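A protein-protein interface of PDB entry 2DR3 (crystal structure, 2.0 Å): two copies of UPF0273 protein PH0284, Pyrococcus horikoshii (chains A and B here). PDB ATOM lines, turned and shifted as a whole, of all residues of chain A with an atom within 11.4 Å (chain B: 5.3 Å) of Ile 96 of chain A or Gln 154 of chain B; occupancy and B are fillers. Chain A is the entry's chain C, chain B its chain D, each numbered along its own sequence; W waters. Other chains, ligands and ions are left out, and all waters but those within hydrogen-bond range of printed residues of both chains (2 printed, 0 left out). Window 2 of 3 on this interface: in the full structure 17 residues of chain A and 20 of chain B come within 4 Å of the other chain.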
ATOM      1  N   ALA A  58      -5.538 -15.482  10.484  1.00  0.00           N
ATOM      2  CA  ALA A  58      -5.359 -15.513   9.039  1.00  0.00           C
ATOM      3  C   ALA A  58      -6.626 -15.757   8.233  1.00  0.00           C
ATOM      4  O   ALA A  58      -7.222 -16.829   8.310  1.00  0.00           O
ATOM      5  CB  ALA A  58      -4.321 -16.569   8.680  1.00  0.00           C
ATOM      6  N   LEU A  59      -7.027 -14.762   7.443  1.00  0.00           N
ATOM      7  CA  LEU A  59      -8.202 -14.901   6.591  1.00  0.00           C
ATOM      8  C   LEU A  59      -7.839 -14.779   5.107  1.00  0.00           C
ATOM      9  O   LEU A  59      -8.678 -15.042   4.237  1.00  0.00           O
ATOM     10  CB  LEU A  59      -9.261 -13.844   6.926  1.00  0.00           C
ATOM     11  CG  LEU A  59     -10.036 -13.966   8.238  1.00  0.00           C
ATOM     12  CD1 LEU A  59      -9.450 -13.028   9.292  1.00  0.00           C
ATOM     13  CD2 LEU A  59     -11.490 -13.622   7.977  1.00  0.00           C
ATOM     14  N   GLU A  60      -6.597 -14.385   4.822  1.00  0.00           N
ATOM     15  CA  GLU A  60      -6.145 -14.198   3.439  1.00  0.00           C
ATOM     16  C   GLU A  60      -5.203 -15.280   2.918  1.00  0.00           C
ATOM     17  O   GLU A  60      -5.154 -15.535   1.713  1.00  0.00           O
ATOM     18  CB  GLU A  60      -5.456 -12.835   3.284  1.00  0.00           C
ATOM     19  CG  GLU A  60      -6.232 -11.655   3.876  1.00  0.00           C
ATOM     20  CD  GLU A  60      -7.681 -11.590   3.422  1.00  0.00           C
ATOM     21  OE1 GLU A  60      -7.939 -11.565   2.192  1.00  0.00           O
ATOM     22  OE2 GLU A  60      -8.564 -11.556   4.306  1.00  0.00           O
ATOM     23  N   GLU A  61      -4.446 -15.898   3.820  1.00  0.00           N
ATOM     24  CA  GLU A  61      -3.504 -16.956   3.459  1.00  0.00           C
ATOM     25  C   GLU A  61      -3.576 -18.025   4.544  1.00  0.00           C
ATOM     26  O   GLU A  61      -4.051 -17.761   5.651  1.00  0.00           O
ATOM     27  CB  GLU A  61      -2.068 -16.419   3.411  1.00  0.00           C
ATOM     28  CG  GLU A  61      -1.819 -15.238   2.490  1.00  0.00           C
ATOM     29  CD  GLU A  61      -0.423 -14.662   2.680  1.00  0.00           C
ATOM     30  OE1 GLU A  61       0.554 -15.433   2.582  1.00  0.00           O
ATOM     31  OE2 GLU A  61      -0.296 -13.440   2.931  1.00  0.00           O
ATOM     32  N   HIS A  62      -3.093 -19.226   4.240  1.00  0.00           N
ATOM     33  CA  HIS A  62      -3.098 -20.307   5.226  1.00  0.00           C
ATOM     34  C   HIS A  62      -1.983 -20.042   6.226  1.00  0.00           C
ATOM     35  O   HIS A  62      -0.916 -19.576   5.852  1.00  0.00           O
ATOM     36  CB  HIS A  62      -2.844 -21.659   4.559  1.00  0.00           C
ATOM     37  CG  HIS A  62      -2.991 -22.821   5.490  1.00  0.00           C
ATOM     38  ND1 HIS A  62      -1.918 -23.392   6.143  1.00  0.00           N
ATOM     39  CD2 HIS A  62      -4.077 -23.542   5.851  1.00  0.00           C
ATOM     40  CE1 HIS A  62      -2.340 -24.416   6.866  1.00  0.00           C
ATOM     41  NE2 HIS A  62      -3.645 -24.529   6.706  1.00  0.00           N
ATOM     42  N   PRO A  63      -2.215 -20.340   7.515  1.00  0.00           N
ATOM     43  CA  PRO A  63      -1.178 -20.109   8.525  1.00  0.00           C
ATOM     44  C   PRO A  63       0.205 -20.601   8.096  1.00  0.00           C
ATOM     45  O   PRO A  63       1.215 -19.947   8.363  1.00  0.00           O
ATOM     46  CB  PRO A  63      -1.719 -20.852   9.737  1.00  0.00           C
ATOM     47  CG  PRO A  63      -3.177 -20.602   9.626  1.00  0.00           C
ATOM     48  CD  PRO A  63      -3.450 -20.839   8.142  1.00  0.00           C
ATOM     49  N   GLN A  65       1.570 -20.597   5.195  1.00  0.00           N
ATOM     50  CA  GLN A  65       2.211 -19.597   4.340  1.00  0.00           C
ATOM     51  C   GLN A  65       2.601 -18.356   5.136  1.00  0.00           C
ATOM     52  O   GLN A  65       3.657 -17.769   4.903  1.00  0.00           O
ATOM     53  CB  GLN A  65       1.293 -19.201   3.180  1.00  0.00           C
ATOM     54  CG  GLN A  65       1.440 -20.089   1.953  1.00  0.00           C
ATOM     55  CD  GLN A  65       1.117 -21.537   2.241  1.00  0.00           C
ATOM     56  OE1 GLN A  65      -0.018 -21.878   2.582  1.00  0.00           O
ATOM     57  NE2 GLN A  65       2.118 -22.402   2.113  1.00  0.00           N
ATOM     58  N   ASP A  90      -6.753 -20.215  11.861  1.00  0.00           N
ATOM     59  CA  ASP A  90      -7.121 -20.460  10.480  1.00  0.00           C
ATOM     60  C   ASP A  90      -8.573 -20.129  10.208  1.00  0.00           C
ATOM     61  O   ASP A  90      -9.459 -20.923  10.511  1.00  0.00           O
ATOM     62  CB  ASP A  90      -6.883 -21.931  10.120  1.00  0.00           C
ATOM     63  CG  ASP A  90      -7.118 -22.226   8.640  1.00  0.00           C
ATOM     64  OD1 ASP A  90      -7.723 -21.394   7.930  1.00  0.00           O
ATOM     65  OD2 ASP A  90      -6.696 -23.309   8.186  1.00  0.00           O
ATOM     66  N   ALA A  91      -8.813 -18.945   9.656  1.00  0.00           N
ATOM     67  CA  ALA A  91     -10.158 -18.539   9.279  1.00  0.00           C
ATOM     68  C   ALA A  91     -10.011 -18.171   7.804  1.00  0.00           C
ATOM     69  O   ALA A  91     -10.629 -17.231   7.314  1.00  0.00           O
ATOM     70  CB  ALA A  91     -10.614 -17.333  10.096  1.00  0.00           C
ATOM     71  N   PHE A  92      -9.164 -18.935   7.119  1.00  0.00           N
ATOM     72  CA  PHE A  92      -8.860 -18.744   5.706  1.00  0.00           C
ATOM     73  C   PHE A  92      -9.448 -19.863   4.850  1.00  0.00           C
ATOM     74  O   PHE A  92     -10.123 -19.616   3.846  1.00  0.00           O
ATOM     75  CB  PHE A  92      -7.343 -18.708   5.531  1.00  0.00           C
ATOM     76  CG  PHE A  92      -6.883 -19.019   4.137  1.00  0.00           C
ATOM     77  CD1 PHE A  92      -6.968 -18.067   3.130  1.00  0.00           C
ATOM     78  CD2 PHE A  92      -6.370 -20.275   3.831  1.00  0.00           C
ATOM     79  CE1 PHE A  92      -6.548 -18.361   1.835  1.00  0.00           C
ATOM     80  CE2 PHE A  92      -5.948 -20.578   2.540  1.00  0.00           C
ATOM     81  CZ  PHE A  92      -6.037 -19.619   1.542  1.00  0.00           C
ATOM     82  N   THR A  93      -9.177 -21.097   5.259  1.00  0.00           N
ATOM     83  CA  THR A  93      -9.653 -22.276   4.553  1.00  0.00           C
ATOM     84  C   THR A  93     -11.169 -22.280   4.343  1.00  0.00           C
ATOM     85  O   THR A  93     -11.650 -22.504   3.229  1.00  0.00           O
ATOM     86  CB  THR A  93      -9.251 -23.559   5.312  1.00  0.00           C
ATOM     87  OG1 THR A  93      -7.820 -23.656   5.368  1.00  0.00           O
ATOM     88  CG2 THR A  93      -9.816 -24.791   4.616  1.00  0.00           C
ATOM     89  N   ALA A  94     -11.920 -22.032   5.413  1.00  0.00           N
ATOM     90  CA  ALA A  94     -13.379 -22.021   5.340  1.00  0.00           C
ATOM     91  C   ALA A  94     -13.920 -21.018   4.331  1.00  0.00           C
ATOM     92  O   ALA A  94     -15.119 -21.006   4.045  1.00  0.00           O
ATOM     93  CB  ALA A  94     -13.966 -21.727   6.712  1.00  0.00           C
ATOM     94  N   GLY A  95     -13.040 -20.176   3.796  1.00  0.00           N
ATOM     95  CA  GLY A  95     -13.477 -19.178   2.835  1.00  0.00           C
ATOM     96  C   GLY A  95     -13.353 -19.596   1.382  1.00  0.00           C
ATOM     97  O   GLY A  95     -14.046 -19.056   0.518  1.00  0.00           O
ATOM     98  N   ILE A  96     -12.480 -20.560   1.108  1.00  0.00           N
ATOM     99  CA  ILE A  96     -12.274 -21.020  -0.257  1.00  0.00           C
ATOM    100  C   ILE A  96     -12.608 -22.495  -0.479  1.00  0.00           C
ATOM    101  O   ILE A  96     -13.243 -22.846  -1.475  1.00  0.00           O
ATOM    102  CB  ILE A  96     -10.823 -20.768  -0.699  1.00  0.00           C
ATOM    103  CG1 ILE A  96      -9.861 -21.561   0.188  1.00  0.00           C
ATOM    104  CG2 ILE A  96     -10.512 -19.280  -0.610  1.00  0.00           C
ATOM    105  CD1 ILE A  96      -8.423 -21.470  -0.249  1.00  0.00           C
ATOM    106  N   GLY A  97     -12.184 -23.355   0.444  1.00  0.00           N
ATOM    107  CA  GLY A  97     -12.461 -24.774   0.295  1.00  0.00           C
ATOM    108  C   GLY A  97     -12.506 -25.556   1.593  1.00  0.00           C
ATOM    109  O   GLY A  97     -13.249 -25.210   2.514  1.00  0.00           O
ATOM    110  N   GLU A 101      -4.563 -30.397   5.824  1.00  0.00           N
ATOM    111  CA  GLU A 101      -3.545 -30.688   6.825  1.00  0.00           C
ATOM    112  C   GLU A 101      -4.075 -30.251   8.196  1.00  0.00           C
ATOM    113  O   GLU A 101      -5.275 -30.013   8.345  1.00  0.00           O
ATOM    114  CB  GLU A 101      -2.239 -29.966   6.468  1.00  0.00           C
ATOM    115  CG  GLU A 101      -2.386 -28.475   6.182  1.00  0.00           C
ATOM    116  CD  GLU A 101      -1.163 -27.885   5.489  1.00  0.00           C
ATOM    117  OE1 GLU A 101      -0.035 -28.073   5.997  1.00  0.00           O
ATOM    118  OE2 GLU A 101      -1.330 -27.230   4.439  1.00  0.00           O
ATOM    119  N   ILE A 106      -8.953 -23.388  14.178  1.00  0.00           N
ATOM    120  CA  ILE A 106      -9.608 -23.288  12.879  1.00  0.00           C
ATOM    121  C   ILE A 106     -11.054 -22.854  13.025  1.00  0.00           C
ATOM    122  O   ILE A 106     -11.747 -23.278  13.951  1.00  0.00           O
ATOM    123  CB  ILE A 106      -9.588 -24.648  12.141  1.00  0.00           C
ATOM    124  CG1 ILE A 106     -10.426 -24.566  10.861  1.00  0.00           C
ATOM    125  CG2 ILE A 106     -10.116 -25.736  13.065  1.00  0.00           C
ATOM    126  CD1 ILE A 106     -10.531 -25.867  10.096  1.00  0.00           C
ATOM    127  N   VAL A 107     -11.496 -21.999  12.108  1.00  0.00           N
ATOM    128  CA  VAL A 107     -12.869 -21.518  12.100  1.00  0.00           C
ATOM    129  C   VAL A 107     -13.515 -22.174  10.888  1.00  0.00           C
ATOM    130  O   VAL A 107     -13.198 -21.830   9.744  1.00  0.00           O
ATOM    131  CB  VAL A 107     -12.922 -19.978  11.960  1.00  0.00           C
ATOM    132  CG1 VAL A 107     -14.330 -19.485  12.193  1.00  0.00           C
ATOM    133  CG2 VAL A 107     -11.959 -19.326  12.952  1.00  0.00           C
ATOM    134  N   HIS A 108     -14.412 -23.126  11.135  1.00  0.00           N
ATOM    135  CA  HIS A 108     -15.073 -23.851  10.052  1.00  0.00           C
ATOM    136  C   HIS A 108     -16.136 -23.064   9.297  1.00  0.00           C
ATOM    137  O   HIS A 108     -16.245 -23.173   8.076  1.00  0.00           O
ATOM    138  CB  HIS A 108     -15.697 -25.143  10.584  1.00  0.00           C
ATOM    139  CG  HIS A 108     -14.706 -26.080  11.198  1.00  0.00           C
ATOM    140  ND1 HIS A 108     -14.352 -27.277  10.614  1.00  0.00           N
ATOM    141  CD2 HIS A 108     -14.014 -26.008  12.360  1.00  0.00           C
ATOM    142  CE1 HIS A 108     -13.485 -27.903  11.391  1.00  0.00           C
ATOM    143  NE2 HIS A 108     -13.264 -27.154  12.456  1.00  0.00           N
ATOM    144  N   ASP A 109     -16.918 -22.276  10.024  1.00  0.00           N
ATOM    145  CA  ASP A 109     -18.000 -21.511   9.405  1.00  0.00           C
ATOM    146  C   ASP A 109     -17.841 -19.999   9.625  1.00  0.00           C
ATOM    147  O   ASP A 109     -17.695 -19.512  10.737  1.00  0.00           O
ATOM    148  CB  ASP A 109     -19.341 -22.012   9.962  1.00  0.00           C
ATOM    149  CG  ASP A 109     -20.444 -21.058   9.522  1.00  0.00           C
ATOM    150  OD1 ASP A 109     -20.585 -20.870   8.315  1.00  0.00           O
ATOM    151  OD2 ASP A 109     -21.181 -20.570  10.379  1.00  0.00           O
ATOM    152  N   LEU A 110     -17.830 -19.262   8.500  1.00  0.00           N
ATOM    153  CA  LEU A 110     -17.691 -17.809   8.572  1.00  0.00           C
ATOM    154  C   LEU A 110     -19.010 -17.094   8.262  1.00  0.00           C
ATOM    155  O   LEU A 110     -19.094 -15.878   8.148  1.00  0.00           O
ATOM    156  CB  LEU A 110     -16.599 -17.382   7.590  1.00  0.00           C
ATOM    157  CG  LEU A 110     -15.193 -17.663   8.130  1.00  0.00           C
ATOM    158  CD1 LEU A 110     -14.091 -17.185   7.180  1.00  0.00           C
ATOM    159  CD2 LEU A 110     -14.924 -16.984   9.473  1.00  0.00           C
ATOM    160  N   THR A 111     -20.063 -17.923   8.084  1.00  0.00           N
ATOM    161  CA  THR A 111     -21.423 -17.409   7.922  1.00  0.00           C
ATOM    162  C   THR A 111     -21.684 -16.220   8.850  1.00  0.00           C
ATOM    163  O   THR A 111     -22.350 -15.251   8.511  1.00  0.00           O
ATOM    164  CB  THR A 111     -22.371 -18.532   8.328  1.00  0.00           C
ATOM    165  OG1 THR A 111     -22.718 -19.309   7.184  1.00  0.00           O
ATOM    166  CG2 THR A 111     -23.641 -17.935   8.939  1.00  0.00           C
ATOM    167  N   THR A 139     -12.645  -9.200   5.155  1.00  0.00           N
ATOM    168  CA  THR A 139     -13.118 -10.465   4.633  1.00  0.00           C
ATOM    169  C   THR A 139     -14.343 -11.002   5.361  1.00  0.00           C
ATOM    170  O   THR A 139     -15.181 -11.668   4.746  1.00  0.00           O
ATOM    171  CB  THR A 139     -11.979 -11.485   4.638  1.00  0.00           C
ATOM    172  OG1 THR A 139     -10.961 -11.021   3.743  1.00  0.00           O
ATOM    173  CG2 THR A 139     -12.460 -12.865   4.173  1.00  0.00           C
ATOM    174  N   ILE A 142     -17.141  -8.652   3.612  1.00  0.00           N
ATOM    175  CA  ILE A 142     -17.017  -8.178   2.242  1.00  0.00           C
ATOM    176  C   ILE A 142     -18.292  -8.332   1.403  1.00  0.00           C
ATOM    177  O   ILE A 142     -18.538  -7.530   0.496  1.00  0.00           O
ATOM    178  CB  ILE A 142     -15.822  -8.866   1.528  1.00  0.00           C
ATOM    179  CG1 ILE A 142     -15.525  -8.151   0.211  1.00  0.00           C
ATOM    180  CG2 ILE A 142     -16.122 -10.340   1.294  1.00  0.00           C
ATOM    181  CD1 ILE A 142     -15.267  -6.652   0.362  1.00  0.00           C
ATOM    182  N   ASN A 143     -19.110  -9.338   1.706  1.00  0.00           N
ATOM    183  CA  ASN A 143     -20.353  -9.540   0.964  1.00  0.00           C
ATOM    184  C   ASN A 143     -21.586  -9.109   1.760  1.00  0.00           C
ATOM    185  O   ASN A 143     -22.712  -9.137   1.248  1.00  0.00           O
ATOM    186  CB  ASN A 143     -20.503 -11.007   0.534  1.00  0.00           C
ATOM    187  CG  ASN A 143     -19.436 -11.437  -0.458  1.00  0.00           C
ATOM    188  OD1 ASN A 143     -19.173 -10.748  -1.447  1.00  0.00           O
ATOM    189  ND2 ASN A 143     -18.821 -12.587  -0.205  1.00  0.00           N
ATOM    190  N   ILE B 113     -15.485 -23.399 -11.359  1.00  0.00           N
ATOM    191  CA  ILE B 113     -14.054 -23.503 -11.649  1.00  0.00           C
ATOM    192  C   ILE B 113     -13.524 -24.881 -11.261  1.00  0.00           C
ATOM    193  O   ILE B 113     -12.328 -25.154 -11.388  1.00  0.00           O
ATOM    194  CB  ILE B 113     -13.275 -22.379 -10.919  1.00  0.00           C
ATOM    195  CG1 ILE B 113     -13.684 -21.018 -11.486  1.00  0.00           C
ATOM    196  CG2 ILE B 113     -11.785 -22.561 -11.090  1.00  0.00           C
ATOM    197  CD1 ILE B 113     -15.163 -20.692 -11.366  1.00  0.00           C
ATOM    198  N   ILE B 117      -9.878 -26.438 -12.665  1.00  0.00           N
ATOM    199  CA  ILE B 117      -8.757 -26.881 -11.838  1.00  0.00           C
ATOM    200  C   ILE B 117      -8.432 -28.342 -12.163  1.00  0.00           C
ATOM    201  O   ILE B 117      -7.266 -28.695 -12.340  1.00  0.00           O
ATOM    202  CB  ILE B 117      -9.110 -26.719 -10.341  1.00  0.00           C
ATOM    203  CG1 ILE B 117      -9.135 -25.229  -9.990  1.00  0.00           C
ATOM    204  CG2 ILE B 117      -8.120 -27.452  -9.478  1.00  0.00           C
ATOM    205  CD1 ILE B 117      -9.678 -24.941  -8.607  1.00  0.00           C
ATOM    206  N   ARG B 149     -12.923 -13.423  -5.624  1.00  0.00           N
ATOM    207  CA  ARG B 149     -12.025 -13.716  -4.505  1.00  0.00           C
ATOM    208  C   ARG B 149     -11.684 -15.198  -4.322  1.00  0.00           C
ATOM    209  O   ARG B 149     -10.511 -15.576  -4.329  1.00  0.00           O
ATOM    210  CB  ARG B 149     -12.599 -13.178  -3.189  1.00  0.00           C
ATOM    211  CG  ARG B 149     -11.677 -13.454  -1.997  1.00  0.00           C
ATOM    212  CD  ARG B 149     -12.133 -12.758  -0.729  1.00  0.00           C
ATOM    213  NE  ARG B 149     -11.114 -12.839   0.322  1.00  0.00           N
ATOM    214  CZ  ARG B 149     -10.845 -13.932   1.029  1.00  0.00           C
ATOM    215  NH1 ARG B 149     -11.519 -15.054   0.814  1.00  0.00           N
ATOM    216  NH2 ARG B 149      -9.899 -13.900   1.956  1.00  0.00           N
ATOM    217  N   SER B 150     -12.704 -16.037  -4.148  1.00  0.00           N
ATOM    218  CA  SER B 150     -12.456 -17.463  -3.949  1.00  0.00           C
ATOM    219  C   SER B 150     -11.812 -18.101  -5.174  1.00  0.00           C
ATOM    220  O   SER B 150     -10.912 -18.933  -5.044  1.00  0.00           O
ATOM    221  CB  SER B 150     -13.753 -18.198  -3.595  1.00  0.00           C
ATOM    222  OG  SER B 150     -14.677 -18.170  -4.662  1.00  0.00           O
ATOM    223  N   ILE B 151     -12.256 -17.702  -6.364  1.00  0.00           N
ATOM    224  CA  ILE B 151     -11.692 -18.262  -7.587  1.00  0.00           C
ATOM    225  C   ILE B 151     -10.205 -17.964  -7.637  1.00  0.00           C
ATOM    226  O   ILE B 151      -9.389 -18.853  -7.879  1.00  0.00           O
ATOM    227  CB  ILE B 151     -12.398 -17.695  -8.854  1.00  0.00           C
ATOM    228  CG1 ILE B 151     -13.821 -18.261  -8.949  1.00  0.00           C
ATOM    229  CG2 ILE B 151     -11.607 -18.041 -10.101  1.00  0.00           C
ATOM    230  CD1 ILE B 151     -14.669 -17.681 -10.092  1.00  0.00           C
ATOM    231  N   ILE B 152      -9.851 -16.706  -7.380  1.00  0.00           N
ATOM    232  CA  ILE B 152      -8.457 -16.291  -7.395  1.00  0.00           C
ATOM    233  C   ILE B 152      -7.624 -17.071  -6.383  1.00  0.00           C
ATOM    234  O   ILE B 152      -6.539 -17.567  -6.702  1.00  0.00           O
ATOM    235  CB  ILE B 152      -8.322 -14.779  -7.067  1.00  0.00           C
ATOM    236  CG1 ILE B 152      -8.780 -13.934  -8.256  1.00  0.00           C
ATOM    237  CG2 ILE B 152      -6.898 -14.456  -6.700  1.00  0.00           C
ATOM    238  CD1 ILE B 152      -7.897 -14.047  -9.457  1.00  0.00           C
ATOM    239  N   LEU B 153      -8.129 -17.169  -5.156  1.00  0.00           N
ATOM    240  CA  LEU B 153      -7.396 -17.865  -4.100  1.00  0.00           C
ATOM    241  C   LEU B 153      -7.340 -19.368  -4.337  1.00  0.00           C
ATOM    242  O   LEU B 153      -6.343 -20.012  -4.019  1.00  0.00           O
ATOM    243  CB  LEU B 153      -8.015 -17.556  -2.727  1.00  0.00           C
ATOM    244  CG  LEU B 153      -7.954 -16.084  -2.287  1.00  0.00           C
ATOM    245  CD1 LEU B 153      -8.604 -15.938  -0.935  1.00  0.00           C
ATOM    246  CD2 LEU B 153      -6.515 -15.589  -2.233  1.00  0.00           C
ATOM    247  N   GLN B 154      -8.403 -19.928  -4.900  1.00  0.00           N
ATOM    248  CA  GLN B 154      -8.414 -21.358  -5.175  1.00  0.00           C
ATOM    249  C   GLN B 154      -7.382 -21.716  -6.229  1.00  0.00           C
ATOM    250  O   GLN B 154      -6.649 -22.695  -6.076  1.00  0.00           O
ATOM    251  CB  GLN B 154      -9.806 -21.810  -5.618  1.00  0.00           C
ATOM    252  CG  GLN B 154     -10.781 -21.916  -4.465  1.00  0.00           C
ATOM    253  CD  GLN B 154     -12.207 -22.089  -4.924  1.00  0.00           C
ATOM    254  OE1 GLN B 154     -12.493 -22.090  -6.122  1.00  0.00           O
ATOM    255  NE2 GLN B 154     -13.115 -22.244  -3.970  1.00  0.00           N
ATOM    256  N   LEU B 155      -7.304 -20.922  -7.293  1.00  0.00           N
ATOM    257  CA  LEU B 155      -6.334 -21.201  -8.345  1.00  0.00           C
ATOM    258  C   LEU B 155      -4.925 -20.981  -7.813  1.00  0.00           C
ATOM    259  O   LEU B 155      -3.999 -21.707  -8.164  1.00  0.00           O
ATOM    260  CB  LEU B 155      -6.586 -20.310  -9.571  1.00  0.00           C
ATOM    261  CG  LEU B 155      -7.923 -20.489 -10.306  1.00  0.00           C
ATOM    262  CD1 LEU B 155      -8.075 -19.418 -11.375  1.00  0.00           C
ATOM    263  CD2 LEU B 155      -7.997 -21.887 -10.932  1.00  0.00           C
ATOM    264  N   LYS B 156      -4.766 -19.974  -6.960  1.00  0.00           N
ATOM    265  CA  LYS B 156      -3.468 -19.661  -6.368  1.00  0.00           C
ATOM    266  C   LYS B 156      -2.899 -20.872  -5.628  1.00  0.00           C
ATOM    267  O   LYS B 156      -1.770 -21.308  -5.865  1.00  0.00           O
ATOM    268  CB  LYS B 156      -3.626 -18.499  -5.384  1.00  0.00           C
ATOM    269  CG  LYS B 156      -2.360 -18.072  -4.672  1.00  0.00           C
ATOM    270  CD  LYS B 156      -2.688 -16.941  -3.706  1.00  0.00           C
ATOM    271  CE  LYS B 156      -1.489 -16.491  -2.913  1.00  0.00           C
ATOM    272  NZ  LYS B 156      -1.907 -15.471  -1.904  1.00  0.00           N
ATOM    273  N   ARG B 157      -3.692 -21.396  -4.709  1.00  0.00           N
ATOM    274  CA  ARG B 157      -3.297 -22.552  -3.915  1.00  0.00           C
ATOM    275  C   ARG B 157      -2.869 -23.692  -4.848  1.00  0.00           C
ATOM    276  O   ARG B 157      -1.790 -24.276  -4.686  1.00  0.00           O
ATOM    277  CB  ARG B 157      -4.483 -22.969  -3.052  1.00  0.00           C
ATOM    278  CG  ARG B 157      -4.235 -24.072  -2.047  1.00  0.00           C
ATOM    279  CD  ARG B 157      -5.561 -24.546  -1.472  1.00  0.00           C
ATOM    280  NE  ARG B 157      -6.452 -25.020  -2.532  1.00  0.00           N
ATOM    281  CZ  ARG B 157      -7.220 -24.237  -3.289  1.00  0.00           C
ATOM    282  NH1 ARG B 157      -7.223 -22.922  -3.101  1.00  0.00           N
ATOM    283  NH2 ARG B 157      -7.968 -24.763  -4.255  1.00  0.00           N
ATOM    284  N   VAL B 158      -3.716 -23.990  -5.832  1.00  0.00           N
ATOM    285  CA  VAL B 158      -3.438 -25.043  -6.804  1.00  0.00           C
ATOM    286  C   VAL B 158      -2.035 -24.929  -7.398  1.00  0.00           C
ATOM    287  O   VAL B 158      -1.210 -25.828  -7.245  1.00  0.00           O
ATOM    288  CB  VAL B 158      -4.447 -25.003  -7.974  1.00  0.00           C
ATOM    289  CG1 VAL B 158      -3.971 -25.913  -9.102  1.00  0.00           C
ATOM    290  CG2 VAL B 158      -5.820 -25.430  -7.491  1.00  0.00           C
HETATM  291  O   HOH W   1     -10.193 -17.268   2.718  1.00  0.00           O
HETATM  292  O   HOH W   2      -3.931 -17.068  -0.125  1.00  0.00           O
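O of Leu 59 of chain A sits at hydrogen-bond distance from NH2 of Arg 149 of chain B, at 2.8 Å.
OE1 of Glu 60 of chain A is in salt-bridge range of NH2 of Arg 149 of chain B (3.1 Å).
The side-chain amide nitrogen of Gln 154 of chain B is in hydrogen-bond range of the backbone carbonyl oxygen of Ile 96 of chain A.
The side-chain hydroxyl (OG1) of Thr 139 of chain A sits at hydrogen-bond distance from the side-chain carboxylate (OE2) of Glu 60 of chain A, at 2.5 Å.
The guanidinium group of Arg 157 of chain B lies within hydrogen-bond range of the backbone carbonyl oxygen of Leu 153 of chain B, at 3.2 Å.
The backbone carbonyl oxygen (O) of Gln 154 of chain B lies close to the guanidinium group (NH1) of Arg 157 of chain B, at 3.0 Å.
Ile 96 of chain A touches Leu 153 of chain B (CG2 to CB, 3.7 Å).
Ile 96 of chain A touches Arg 157 of chain B (CD1 to NH1, 3.4 Å).
Thr 139 of chain A touches Arg 149 of chain B.
Printed residues of chain B within 4 Å of Leu 59 of chain A: Arg 149.
Of the printed residues of chain B, Ile 96 of chain A touches Leu 153 (3.7 Å), Gln 154 (2.6 Å) and Arg 157 (3.4 Å).
Of the printed residues of chain B, Thr 139 of chain A touches Arg 149.
No residue of chain A comes within 4 Å of Ile 113 of chain B.
Of the printed residues of chain A, Arg 149 of chain B touches Leu 59, Glu 60 and Thr 139.
Ser 150 of chain B touches none of the printed residues of chain A.
Of the printed residues of chain A, Leu 153 of chain B touches Ile 96.
No residue of chain A comes within 4 Å of Leu 155 of chain B.
No residue of chain A comes within 4 Å of Val 158 of chain B.
The nearest printed residue of chain A that does not touch Arg 149 of chain B is Ile 96 of chain A (4.6 Å).
Of the 12 printed residues of chain B, 4 touch a printed residue of chain A.
Hydrophobic or aromatic side chains of chain B within 4 Å of the printed part of chain A: Leu 153.
Printed residues of chain A that touch a printed residue of chain B: Leu 59, Glu 60, Ile 96 and Thr 139.
Hydrophobic or aromatic side chains of chain A within 4 Å of the printed part of chain B: Ile 96.
No position is printed for both chains.
Of the 6 pairs that touch across the chains among the printed residues, none has its exchanged pair printed and touching as well.
Water W1 lies within hydrogen-bond range of the backbone carbonyl oxygen (O) of Phe 92 of chain A (2.6 Å), the backbone carbonyl oxygen (O) of Leu 59 of chain A (3.1 Å) and the guanidinium group (NH1) of Arg 149 of chain B (3.2 Å).
Water W2 lies within hydrogen-bond range of the backbone carbonyl oxygen (O) of Glu 60 of chain A (2.7 Å) and the side-chain amino group (NZ) of Lys 156 of chain B (3.1 Å).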
